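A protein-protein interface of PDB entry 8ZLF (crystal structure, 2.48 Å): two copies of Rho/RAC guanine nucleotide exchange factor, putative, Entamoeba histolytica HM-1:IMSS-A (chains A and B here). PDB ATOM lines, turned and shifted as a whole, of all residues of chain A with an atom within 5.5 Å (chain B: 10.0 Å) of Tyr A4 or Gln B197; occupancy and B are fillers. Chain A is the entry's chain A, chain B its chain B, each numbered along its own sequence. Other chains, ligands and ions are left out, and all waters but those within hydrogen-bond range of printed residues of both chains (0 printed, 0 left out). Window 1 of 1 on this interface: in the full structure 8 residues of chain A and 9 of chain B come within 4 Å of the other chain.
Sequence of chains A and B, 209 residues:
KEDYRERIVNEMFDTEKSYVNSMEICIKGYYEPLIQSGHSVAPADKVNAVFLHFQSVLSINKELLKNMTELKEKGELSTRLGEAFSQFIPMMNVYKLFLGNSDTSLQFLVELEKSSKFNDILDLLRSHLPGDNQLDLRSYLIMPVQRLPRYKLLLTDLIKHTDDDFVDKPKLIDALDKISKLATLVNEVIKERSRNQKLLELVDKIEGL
OD2 of Asp B136 lies within salt-bridge range of NE of Arg A7 (2.8 Å).
ND2 of Asn B196 lies close to NH1 of Arg B138 (2.9 Å).
OD2 of Asp A157 is in hydrogen-bond range of OH of Tyr A4 (2.5 Å).
OE1 of Glu B113 lies within salt-bridge range of NH2 of Arg B138, 2.5 Å away.
Leu B200 touches Lys A1 (CD2 to CG, 3.9 Å).
OH of Tyr A4 touches NE2 of Gln B197, at 3.7 Å.
Arg A7 touches Arg B138 (NH1 to CB, 3.98 Å).
Lys A1 touches just one residue of chain B: Leu B200 (3.9 Å).
No residue of chain B comes within 4 Å of Glu A2.
No residue of chain B comes within 4 Å of Asp A3.
Tyr A4 touches one residue of chain B.
Printed residues of chain B within 4 Å of Arg A7: Asp B136 (2.8 Å) and Arg B138 (3.98 Å).
Printed residues of chain A within 4 Å of Asp B136: Arg A7.
Gln B197 touches just one residue of chain A: Tyr A4.
Of the printed residues of chain A, Leu B200 touches Lys A1 (3.9 Å).
The nearest residue of chain B that does not touch Tyr A4 is Asn B196 (4.6 Å).
The nearest printed residue of chain A that does not touch Leu B200 is His A161 (5.9 Å).
Of the 23 printed residues of chain B, 4 touch a printed residue of chain A.
Hydrophobic or aromatic side chains of chain B within 4 Å of the printed part of chain A: Leu B200.
Along chain B the printed residues that touch a printed residue of chain A span positions 136 to 200.
Among the printed residues, 4 pairs touch across the chains.
Among the printed residues, Asp or Glu carboxylates within 4 Å of a Lys or Arg side-chain nitrogen of the other chain: Arg A7 with Asp B136.
No position is printed for both chains.
Of the 4 pairs that touch across the chains among the printed residues, none has its exchanged pair printed and touching as well.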
ATOM      1  N   LYS A   1       3.723 -14.165 -19.088  1.00  0.00           N
ATOM      2  CA  LYS A   1       4.987 -13.502 -19.528  1.00  0.00           C
ATOM      3  C   LYS A   1       5.837 -14.470 -20.356  1.00  0.00           C
ATOM      4  O   LYS A   1       6.423 -14.074 -21.355  1.00  0.00           O
ATOM      5  CB  LYS A   1       5.770 -12.956 -18.326  1.00  0.00           C
ATOM      6  CG  LYS A   1       6.895 -11.975 -18.653  1.00  0.00           C
ATOM      7  N   GLU A   2       5.886 -15.751 -19.971  1.00  0.00           N
ATOM      8  CA  GLU A   2       6.572 -16.758 -20.770  1.00  0.00           C
ATOM      9  C   GLU A   2       5.868 -16.923 -22.107  1.00  0.00           C
ATOM     10  O   GLU A   2       6.514 -17.166 -23.127  1.00  0.00           O
ATOM     11  CB  GLU A   2       6.627 -18.121 -20.075  1.00  0.00           C
ATOM     12  N   ASP A   3       4.536 -16.794 -22.094  1.00  0.00           N
ATOM     13  CA  ASP A   3       3.739 -17.077 -23.275  1.00  0.00           C
ATOM     14  C   ASP A   3       3.718 -15.849 -24.182  1.00  0.00           C
ATOM     15  O   ASP A   3       3.555 -15.979 -25.381  1.00  0.00           O
ATOM     16  CB  ASP A   3       2.360 -17.602 -22.880  1.00  0.00           C
ATOM     17  CG  ASP A   3       2.397 -18.984 -22.231  1.00  0.00           C
ATOM     18  OD1 ASP A   3       2.532 -19.993 -22.970  1.00  0.00           O
ATOM     19  OD2 ASP A   3       2.320 -19.050 -20.982  1.00  0.00           O
ATOM     20  N   TYR A   4       3.921 -14.657 -23.628  1.00  0.00           N
ATOM     21  CA  TYR A   4       4.142 -13.479 -24.443  1.00  0.00           C
ATOM     22  C   TYR A   4       5.424 -13.647 -25.241  1.00  0.00           C
ATOM     23  O   TYR A   4       5.491 -13.316 -26.429  1.00  0.00           O
ATOM     24  CB  TYR A   4       4.246 -12.244 -23.550  1.00  0.00           C
ATOM     25  CG  TYR A   4       4.488 -10.951 -24.274  1.00  0.00           C
ATOM     26  CD1 TYR A   4       3.491 -10.319 -24.994  1.00  0.00           C
ATOM     27  CD2 TYR A   4       5.741 -10.393 -24.303  1.00  0.00           C
ATOM     28  CE1 TYR A   4       3.711  -9.126 -25.663  1.00  0.00           C
ATOM     29  CE2 TYR A   4       5.984  -9.205 -24.973  1.00  0.00           C
ATOM     30  CZ  TYR A   4       4.966  -8.558 -25.644  1.00  0.00           C
ATOM     31  OH  TYR A   4       5.254  -7.384 -26.291  1.00  0.00           O
ATOM     32  N   ARG A   5       6.456 -14.129 -24.546  1.00  0.00           N
ATOM     33  CA  ARG A   5       7.777 -14.350 -25.116  1.00  0.00           C
ATOM     34  C   ARG A   5       7.654 -15.331 -26.282  1.00  0.00           C
ATOM     35  O   ARG A   5       8.140 -15.065 -27.385  1.00  0.00           O
ATOM     36  CB  ARG A   5       8.707 -14.859 -24.006  1.00  0.00           C
ATOM     37  CG  ARG A   5      10.192 -14.885 -24.335  1.00  0.00           C
ATOM     38  CD  ARG A   5      11.048 -15.441 -23.213  1.00  0.00           C
ATOM     39  NE  ARG A   5      12.462 -15.318 -23.566  1.00  0.00           N
ATOM     40  CZ  ARG A   5      13.115 -16.097 -24.424  1.00  0.00           C
ATOM     41  NH1 ARG A   5      12.587 -17.223 -24.879  1.00  0.00           N
ATOM     42  NH2 ARG A   5      14.343 -15.775 -24.784  1.00  0.00           N
ATOM     43  N   GLU A   6       6.974 -16.450 -26.027  1.00  0.00           N
ATOM     44  CA  GLU A   6       6.792 -17.472 -27.037  1.00  0.00           C
ATOM     45  C   GLU A   6       6.280 -16.843 -28.335  1.00  0.00           C
ATOM     46  O   GLU A   6       6.787 -17.152 -29.416  1.00  0.00           O
ATOM     47  CB  GLU A   6       5.877 -18.582 -26.512  1.00  0.00           C
ATOM     48  CG  GLU A   6       6.319 -19.959 -26.981  1.00  0.00           C
ATOM     49  CD  GLU A   6       7.508 -20.541 -26.220  1.00  0.00           C
ATOM     50  OE1 GLU A   6       8.470 -19.795 -25.950  1.00  0.00           O
ATOM     51  OE2 GLU A   6       7.508 -21.759 -25.915  1.00  0.00           O
ATOM     52  N   ARG A   7       5.305 -15.931 -28.228  1.00  0.00           N
ATOM     53  CA  ARG A   7       4.724 -15.273 -29.391  1.00  0.00           C
ATOM     54  C   ARG A   7       5.803 -14.614 -30.255  1.00  0.00           C
ATOM     55  O   ARG A   7       5.907 -14.866 -31.449  1.00  0.00           O
ATOM     56  CB  ARG A   7       3.729 -14.193 -28.956  1.00  0.00           C
ATOM     57  CG  ARG A   7       2.306 -14.681 -28.765  1.00  0.00           C
ATOM     58  CD  ARG A   7       1.308 -13.534 -28.826  1.00  0.00           C
ATOM     59  NE  ARG A   7       0.864 -13.217 -30.182  1.00  0.00           N
ATOM     60  CZ  ARG A   7       0.650 -11.988 -30.648  1.00  0.00           C
ATOM     61  NH1 ARG A   7      -0.002 -11.814 -31.790  1.00  0.00           N
ATOM     62  NH2 ARG A   7       1.023 -10.933 -29.937  1.00  0.00           N
ATOM     63  N   ILE A   8       6.606 -13.745 -29.637  1.00  0.00           N
ATOM     64  CA  ILE A   8       7.668 -13.037 -30.332  1.00  0.00           C
ATOM     65  C   ILE A   8       8.592 -14.020 -31.030  1.00  0.00           C
ATOM     66  O   ILE A   8       8.888 -13.850 -32.194  1.00  0.00           O
ATOM     67  CB  ILE A   8       8.460 -12.162 -29.353  1.00  0.00           C
ATOM     68  CG1 ILE A   8       7.559 -11.092 -28.744  1.00  0.00           C
ATOM     69  CG2 ILE A   8       9.672 -11.561 -30.035  1.00  0.00           C
ATOM     70  CD1 ILE A   8       8.115 -10.531 -27.485  1.00  0.00           C
ATOM     71  N   ASP A 157      11.865  -6.378 -27.934  1.00  0.00           N
ATOM     72  CA  ASP A 157      10.730  -6.873 -27.170  1.00  0.00           C
ATOM     73  C   ASP A 157      11.048  -8.231 -26.534  1.00  0.00           C
ATOM     74  O   ASP A 157      10.575  -8.535 -25.442  1.00  0.00           O
ATOM     75  CB  ASP A 157       9.471  -6.912 -28.049  1.00  0.00           C
ATOM     76  CG  ASP A 157       8.174  -6.890 -27.271  1.00  0.00           C
ATOM     77  OD1 ASP A 157       8.070  -6.083 -26.270  1.00  0.00           O
ATOM     78  OD2 ASP A 157       7.262  -7.644 -27.686  1.00  0.00           O
ATOM     79  N   HIS A 161      11.689  -9.270 -22.334  1.00  0.00           N
ATOM     80  CA  HIS A 161      10.863 -10.334 -21.798  1.00  0.00           C
ATOM     81  C   HIS A 161      11.661 -11.610 -21.566  1.00  0.00           C
ATOM     82  O   HIS A 161      11.097 -12.693 -21.473  1.00  0.00           O
ATOM     83  CB  HIS A 161       9.687 -10.564 -22.733  1.00  0.00           C
ATOM     84  CG  HIS A 161       8.927  -9.294 -22.825  1.00  0.00           C
ATOM     85  ND1 HIS A 161       9.417  -8.136 -23.395  1.00  0.00           N
ATOM     86  CD2 HIS A 161       7.734  -9.004 -22.346  1.00  0.00           C
ATOM     87  CE1 HIS A 161       8.511  -7.190 -23.299  1.00  0.00           C
ATOM     88  NE2 HIS A 161       7.485  -7.690 -22.637  1.00  0.00           N
ATOM     89  N   LEU B 106     -10.273  -8.340 -24.786  1.00  0.00           N
ATOM     90  CA  LEU B 106      -8.954  -8.779 -24.360  1.00  0.00           C
ATOM     91  C   LEU B 106      -8.980  -9.222 -22.905  1.00  0.00           C
ATOM     92  O   LEU B 106      -8.267 -10.156 -22.540  1.00  0.00           O
ATOM     93  CB  LEU B 106      -7.913  -7.679 -24.536  1.00  0.00           C
ATOM     94  CG  LEU B 106      -6.487  -8.114 -24.186  1.00  0.00           C
ATOM     95  CD1 LEU B 106      -6.042  -9.283 -25.064  1.00  0.00           C
ATOM     96  CD2 LEU B 106      -5.492  -6.955 -24.322  1.00  0.00           C
ATOM     97  N   GLN B 107      -9.761  -8.533 -22.066  1.00  0.00           N
ATOM     98  CA  GLN B 107      -9.859  -8.923 -20.676  1.00  0.00           C
ATOM     99  C   GLN B 107     -10.422 -10.350 -20.584  1.00  0.00           C
ATOM    100  O   GLN B 107      -9.964 -11.178 -19.783  1.00  0.00           O
ATOM    101  CB  GLN B 107     -10.691  -7.889 -19.917  1.00  0.00           C
ATOM    102  CG  GLN B 107     -10.842  -8.163 -18.424  1.00  0.00           C
ATOM    103  CD  GLN B 107      -9.511  -8.312 -17.724  1.00  0.00           C
ATOM    104  OE1 GLN B 107      -8.578  -7.552 -17.982  1.00  0.00           O
ATOM    105  NE2 GLN B 107      -9.400  -9.319 -16.859  1.00  0.00           N
ATOM    106  N   VAL B 110      -7.697 -13.031 -21.746  1.00  0.00           N
ATOM    107  CA  VAL B 110      -6.609 -13.192 -20.802  1.00  0.00           C
ATOM    108  C   VAL B 110      -7.107 -14.006 -19.620  1.00  0.00           C
ATOM    109  O   VAL B 110      -6.316 -14.700 -19.012  1.00  0.00           O
ATOM    110  CB  VAL B 110      -6.086 -11.811 -20.344  1.00  0.00           C
ATOM    111  CG1 VAL B 110      -5.321 -11.868 -19.039  1.00  0.00           C
ATOM    112  CG2 VAL B 110      -5.248 -11.135 -21.414  1.00  0.00           C
ATOM    113  N   GLU B 113      -7.281 -17.501 -20.730  1.00  0.00           N
ATOM    114  CA  GLU B 113      -5.948 -17.985 -21.051  1.00  0.00           C
ATOM    115  C   GLU B 113      -5.160 -18.317 -19.789  1.00  0.00           C
ATOM    116  O   GLU B 113      -3.972 -18.622 -19.859  1.00  0.00           O
ATOM    117  CB  GLU B 113      -5.191 -16.956 -21.898  1.00  0.00           C
ATOM    118  CG  GLU B 113      -5.511 -17.018 -23.387  1.00  0.00           C
ATOM    119  CD  GLU B 113      -5.070 -15.800 -24.186  1.00  0.00           C
ATOM    120  OE1 GLU B 113      -4.661 -14.800 -23.536  1.00  0.00           O
ATOM    121  OE2 GLU B 113      -5.152 -15.835 -25.455  1.00  0.00           O
ATOM    122  N   LYS B 114      -5.808 -18.249 -18.630  1.00  0.00           N
ATOM    123  CA  LYS B 114      -5.229 -18.804 -17.415  1.00  0.00           C
ATOM    124  C   LYS B 114      -5.326 -20.326 -17.452  1.00  0.00           C
ATOM    125  O   LYS B 114      -4.443 -21.019 -16.932  1.00  0.00           O
ATOM    126  CB  LYS B 114      -5.935 -18.261 -16.178  1.00  0.00           C
ATOM    127  CG  LYS B 114      -5.839 -16.753 -16.023  1.00  0.00           C
ATOM    128  CD  LYS B 114      -4.430 -16.193 -15.933  1.00  0.00           C
ATOM    129  CE  LYS B 114      -4.468 -14.683 -15.836  1.00  0.00           C
ATOM    130  NZ  LYS B 114      -3.282 -14.107 -15.161  1.00  0.00           N
ATOM    131  N   ASN B 119      -5.683 -23.037 -23.421  1.00  0.00           N
ATOM    132  CA  ASN B 119      -4.548 -22.761 -24.287  1.00  0.00           C
ATOM    133  C   ASN B 119      -4.280 -23.912 -25.260  1.00  0.00           C
ATOM    134  O   ASN B 119      -3.971 -23.671 -26.427  1.00  0.00           O
ATOM    135  CB  ASN B 119      -3.304 -22.397 -23.483  1.00  0.00           C
ATOM    136  CG  ASN B 119      -3.348 -20.971 -22.997  1.00  0.00           C
ATOM    137  OD1 ASN B 119      -3.593 -20.064 -23.785  1.00  0.00           O
ATOM    138  ND2 ASN B 119      -3.136 -20.758 -21.712  1.00  0.00           N
ATOM    139  N   ASP B 136      -2.065 -16.834 -34.382  1.00  0.00           N
ATOM    140  CA  ASP B 136      -2.791 -16.931 -33.133  1.00  0.00           C
ATOM    141  C   ASP B 136      -4.006 -15.999 -33.180  1.00  0.00           C
ATOM    142  O   ASP B 136      -4.183 -15.203 -34.107  1.00  0.00           O
ATOM    143  CB  ASP B 136      -1.874 -16.599 -31.955  1.00  0.00           C
ATOM    144  CG  ASP B 136      -1.337 -15.178 -31.980  1.00  0.00           C
ATOM    145  OD1 ASP B 136      -0.814 -14.754 -33.049  1.00  0.00           O
ATOM    146  OD2 ASP B 136      -1.498 -14.492 -30.951  1.00  0.00           O
ATOM    147  N   ARG B 138      -5.037 -13.397 -31.112  1.00  0.00           N
ATOM    148  CA  ARG B 138      -4.798 -11.965 -30.966  1.00  0.00           C
ATOM    149  C   ARG B 138      -4.448 -11.349 -32.312  1.00  0.00           C
ATOM    150  O   ARG B 138      -4.829 -10.235 -32.663  1.00  0.00           O
ATOM    151  CB  ARG B 138      -3.588 -11.702 -30.070  1.00  0.00           C
ATOM    152  CG  ARG B 138      -3.861 -11.932 -28.598  1.00  0.00           C
ATOM    153  CD  ARG B 138      -2.635 -12.475 -27.910  1.00  0.00           C
ATOM    154  NE  ARG B 138      -3.007 -12.953 -26.598  1.00  0.00           N
ATOM    155  CZ  ARG B 138      -3.227 -12.180 -25.545  1.00  0.00           C
ATOM    156  NH1 ARG B 138      -3.046 -10.872 -25.609  1.00  0.00           N
ATOM    157  NH2 ARG B 138      -3.611 -12.722 -24.404  1.00  0.00           N
ATOM    158  N   VAL B 189      -4.975   0.839 -29.043  1.00  0.00           N
ATOM    159  CA  VAL B 189      -3.653   0.229 -29.007  1.00  0.00           C
ATOM    160  C   VAL B 189      -3.057   0.397 -27.606  1.00  0.00           C
ATOM    161  O   VAL B 189      -2.614  -0.581 -27.001  1.00  0.00           O
ATOM    162  CB  VAL B 189      -2.739   0.798 -30.111  1.00  0.00           C
ATOM    163  CG1 VAL B 189      -1.272   0.508 -29.842  1.00  0.00           C
ATOM    164  CG2 VAL B 189      -3.116   0.291 -31.498  1.00  0.00           C
ATOM    165  N   ILE B 190      -3.110   1.623 -27.069  1.00  0.00           N
ATOM    166  CA  ILE B 190      -2.550   1.906 -25.758  1.00  0.00           C
ATOM    167  C   ILE B 190      -3.167   0.972 -24.716  1.00  0.00           C
ATOM    168  O   ILE B 190      -2.433   0.326 -23.962  1.00  0.00           O
ATOM    169  CB  ILE B 190      -2.706   3.393 -25.374  1.00  0.00           C
ATOM    170  N   LYS B 191      -4.502   0.872 -24.692  1.00  0.00           N
ATOM    171  CA  LYS B 191      -5.187   0.194 -23.602  1.00  0.00           C
ATOM    172  C   LYS B 191      -4.949  -1.311 -23.713  1.00  0.00           C
ATOM    173  O   LYS B 191      -4.834  -1.962 -22.681  1.00  0.00           O
ATOM    174  CB  LYS B 191      -6.670   0.574 -23.566  1.00  0.00           C
ATOM    175  N   GLU B 192      -4.809  -1.836 -24.946  1.00  0.00           N
ATOM    176  CA  GLU B 192      -4.483  -3.242 -25.176  1.00  0.00           C
ATOM    177  C   GLU B 192      -3.065  -3.546 -24.685  1.00  0.00           C
ATOM    178  O   GLU B 192      -2.840  -4.601 -24.088  1.00  0.00           O
ATOM    179  CB  GLU B 192      -4.646  -3.608 -26.654  1.00  0.00           C
ATOM    180  N   ARG B 193      -2.144  -2.588 -24.890  1.00  0.00           N
ATOM    181  CA  ARG B 193      -0.771  -2.714 -24.428  1.00  0.00           C
ATOM    182  C   ARG B 193      -0.762  -2.931 -22.912  1.00  0.00           C
ATOM    183  O   ARG B 193      -0.264  -3.953 -22.426  1.00  0.00           O
ATOM    184  CB  ARG B 193       0.052  -1.482 -24.837  1.00  0.00           C
ATOM    185  CG  ARG B 193       1.566  -1.694 -24.781  1.00  0.00           C
ATOM    186  N   SER B 194      -1.415  -1.998 -22.190  1.00  0.00           N
ATOM    187  CA  SER B 194      -1.391  -1.971 -20.733  1.00  0.00           C
ATOM    188  C   SER B 194      -1.875  -3.307 -20.180  1.00  0.00           C
ATOM    189  O   SER B 194      -1.231  -3.862 -19.291  1.00  0.00           O
ATOM    190  CB  SER B 194      -2.225  -0.849 -20.145  1.00  0.00           C
ATOM    191  OG  SER B 194      -2.075   0.367 -20.867  1.00  0.00           O
ATOM    192  N   ARG B 195      -3.020  -3.788 -20.695  1.00  0.00           N
ATOM    193  CA  ARG B 195      -3.666  -4.992 -20.183  1.00  0.00           C
ATOM    194  C   ARG B 195      -2.742  -6.199 -20.381  1.00  0.00           C
ATOM    195  O   ARG B 195      -2.559  -6.979 -19.455  1.00  0.00           O
ATOM    196  CB  ARG B 195      -5.046  -5.183 -20.828  1.00  0.00           C
ATOM    197  N   ASN B 196      -2.101  -6.282 -21.556  1.00  0.00           N
ATOM    198  CA  ASN B 196      -1.222  -7.381 -21.929  1.00  0.00           C
ATOM    199  C   ASN B 196       0.026  -7.418 -21.035  1.00  0.00           C
ATOM    200  O   ASN B 196       0.676  -8.446 -20.845  1.00  0.00           O
ATOM    201  CB  ASN B 196      -0.820  -7.268 -23.405  1.00  0.00           C
ATOM    202  CG  ASN B 196      -1.113  -8.517 -24.208  1.00  0.00           C
ATOM    203  OD1 ASN B 196      -0.858  -9.630 -23.756  1.00  0.00           O
ATOM    204  ND2 ASN B 196      -1.670  -8.347 -25.398  1.00  0.00           N
ATOM    205  N   GLN B 197       0.396  -6.284 -20.470  1.00  0.00           N
ATOM    206  CA  GLN B 197       1.654  -6.226 -19.761  1.00  0.00           C
ATOM    207  C   GLN B 197       1.436  -5.913 -18.283  1.00  0.00           C
ATOM    208  O   GLN B 197       2.412  -5.716 -17.575  1.00  0.00           O
ATOM    209  CB  GLN B 197       2.506  -5.210 -20.510  1.00  0.00           C
ATOM    210  CG  GLN B 197       2.366  -5.425 -22.007  1.00  0.00           C
ATOM    211  CD  GLN B 197       3.156  -4.463 -22.839  1.00  0.00           C
ATOM    212  OE1 GLN B 197       3.288  -3.281 -22.524  1.00  0.00           O
ATOM    213  NE2 GLN B 197       3.734  -5.001 -23.895  1.00  0.00           N
ATOM    214  N   LYS B 198       0.178  -5.907 -17.816  1.00  0.00           N
ATOM    215  CA  LYS B 198      -0.121  -5.503 -16.455  1.00  0.00           C
ATOM    216  C   LYS B 198       0.603  -6.402 -15.463  1.00  0.00           C
ATOM    217  O   LYS B 198       1.011  -5.929 -14.408  1.00  0.00           O
ATOM    218  CB  LYS B 198      -1.626  -5.515 -16.158  1.00  0.00           C
ATOM    219  CG  LYS B 198      -2.272  -4.144 -15.957  1.00  0.00           C
ATOM    220  CD  LYS B 198      -2.371  -3.666 -14.516  1.00  0.00           C
ATOM    221  CE  LYS B 198      -3.745  -3.833 -13.891  1.00  0.00           C
ATOM    222  NZ  LYS B 198      -4.053  -5.241 -13.530  1.00  0.00           N
ATOM    223  N   LEU B 199       0.749  -7.685 -15.795  1.00  0.00           N
ATOM    224  CA  LEU B 199       1.231  -8.656 -14.830  1.00  0.00           C
ATOM    225  C   LEU B 199       2.680  -9.061 -15.114  1.00  0.00           C
ATOM    226  O   LEU B 199       3.033 -10.210 -14.892  1.00  0.00           O
ATOM    227  CB  LEU B 199       0.295  -9.870 -14.843  1.00  0.00           C
ATOM    228  N   LEU B 200       3.538  -8.124 -15.542  1.00  0.00           N
ATOM    229  CA  LEU B 200       4.982  -8.315 -15.433  1.00  0.00           C
ATOM    230  C   LEU B 200       5.399  -8.292 -13.964  1.00  0.00           C
ATOM    231  O   LEU B 200       5.993  -9.251 -13.479  1.00  0.00           O
ATOM    232  CB  LEU B 200       5.736  -7.225 -16.199  1.00  0.00           C
ATOM    233  CG  LEU B 200       7.259  -7.389 -16.282  1.00  0.00           C
ATOM    234  CD1 LEU B 200       8.000  -6.738 -15.104  1.00  0.00           C
ATOM    235  CD2 LEU B 200       7.648  -8.861 -16.426  1.00  0.00           C
ATOM    236  N   GLU B 201       5.080  -7.193 -13.266  1.00  0.00           N
ATOM    237  CA  GLU B 201       5.438  -7.032 -11.864  1.00  0.00           C
ATOM    238  C   GLU B 201       4.568  -7.970 -11.023  1.00  0.00           C
ATOM    239  O   GLU B 201       5.100  -8.945 -10.483  1.00  0.00           O
ATOM    240  CB  GLU B 201       5.370  -5.561 -11.433  1.00  0.00           C
ATOM    241  N   LEU B 202       3.252  -7.711 -10.893  1.00  0.00           N
ATOM    242  CA  LEU B 202       2.442  -8.621 -10.085  1.00  0.00           C
ATOM    243  C   LEU B 202       1.180  -9.011 -10.817  1.00  0.00           C
ATOM    244  O   LEU B 202       1.127 -10.046 -11.444  1.00  0.00           O
ATOM    245  CB  LEU B 202       2.156  -8.075  -8.674  1.00  0.00           C
ATOM    246  CG  LEU B 202       1.698  -9.115  -7.640  1.00  0.00           C
ATOM    247  CD1 LEU B 202       2.658 -10.305  -7.602  1.00  0.00           C
ATOM    248  CD2 LEU B 202       1.570  -8.491  -6.253  1.00  0.00           C
ATOM    249  N   VAL B 203       0.170  -8.254 -10.691  1.00  0.00           N
ATOM    250  CA  VAL B 203      -1.095  -8.686 -11.204  1.00  0.00           C
ATOM    251  C   VAL B 203      -1.357  -8.032 -12.572  1.00  0.00           C
ATOM    252  O   VAL B 203      -2.326  -8.455 -13.274  1.00  0.00           O
ATOM    253  CB  VAL B 203      -2.196  -8.390 -10.163  1.00  0.00           C
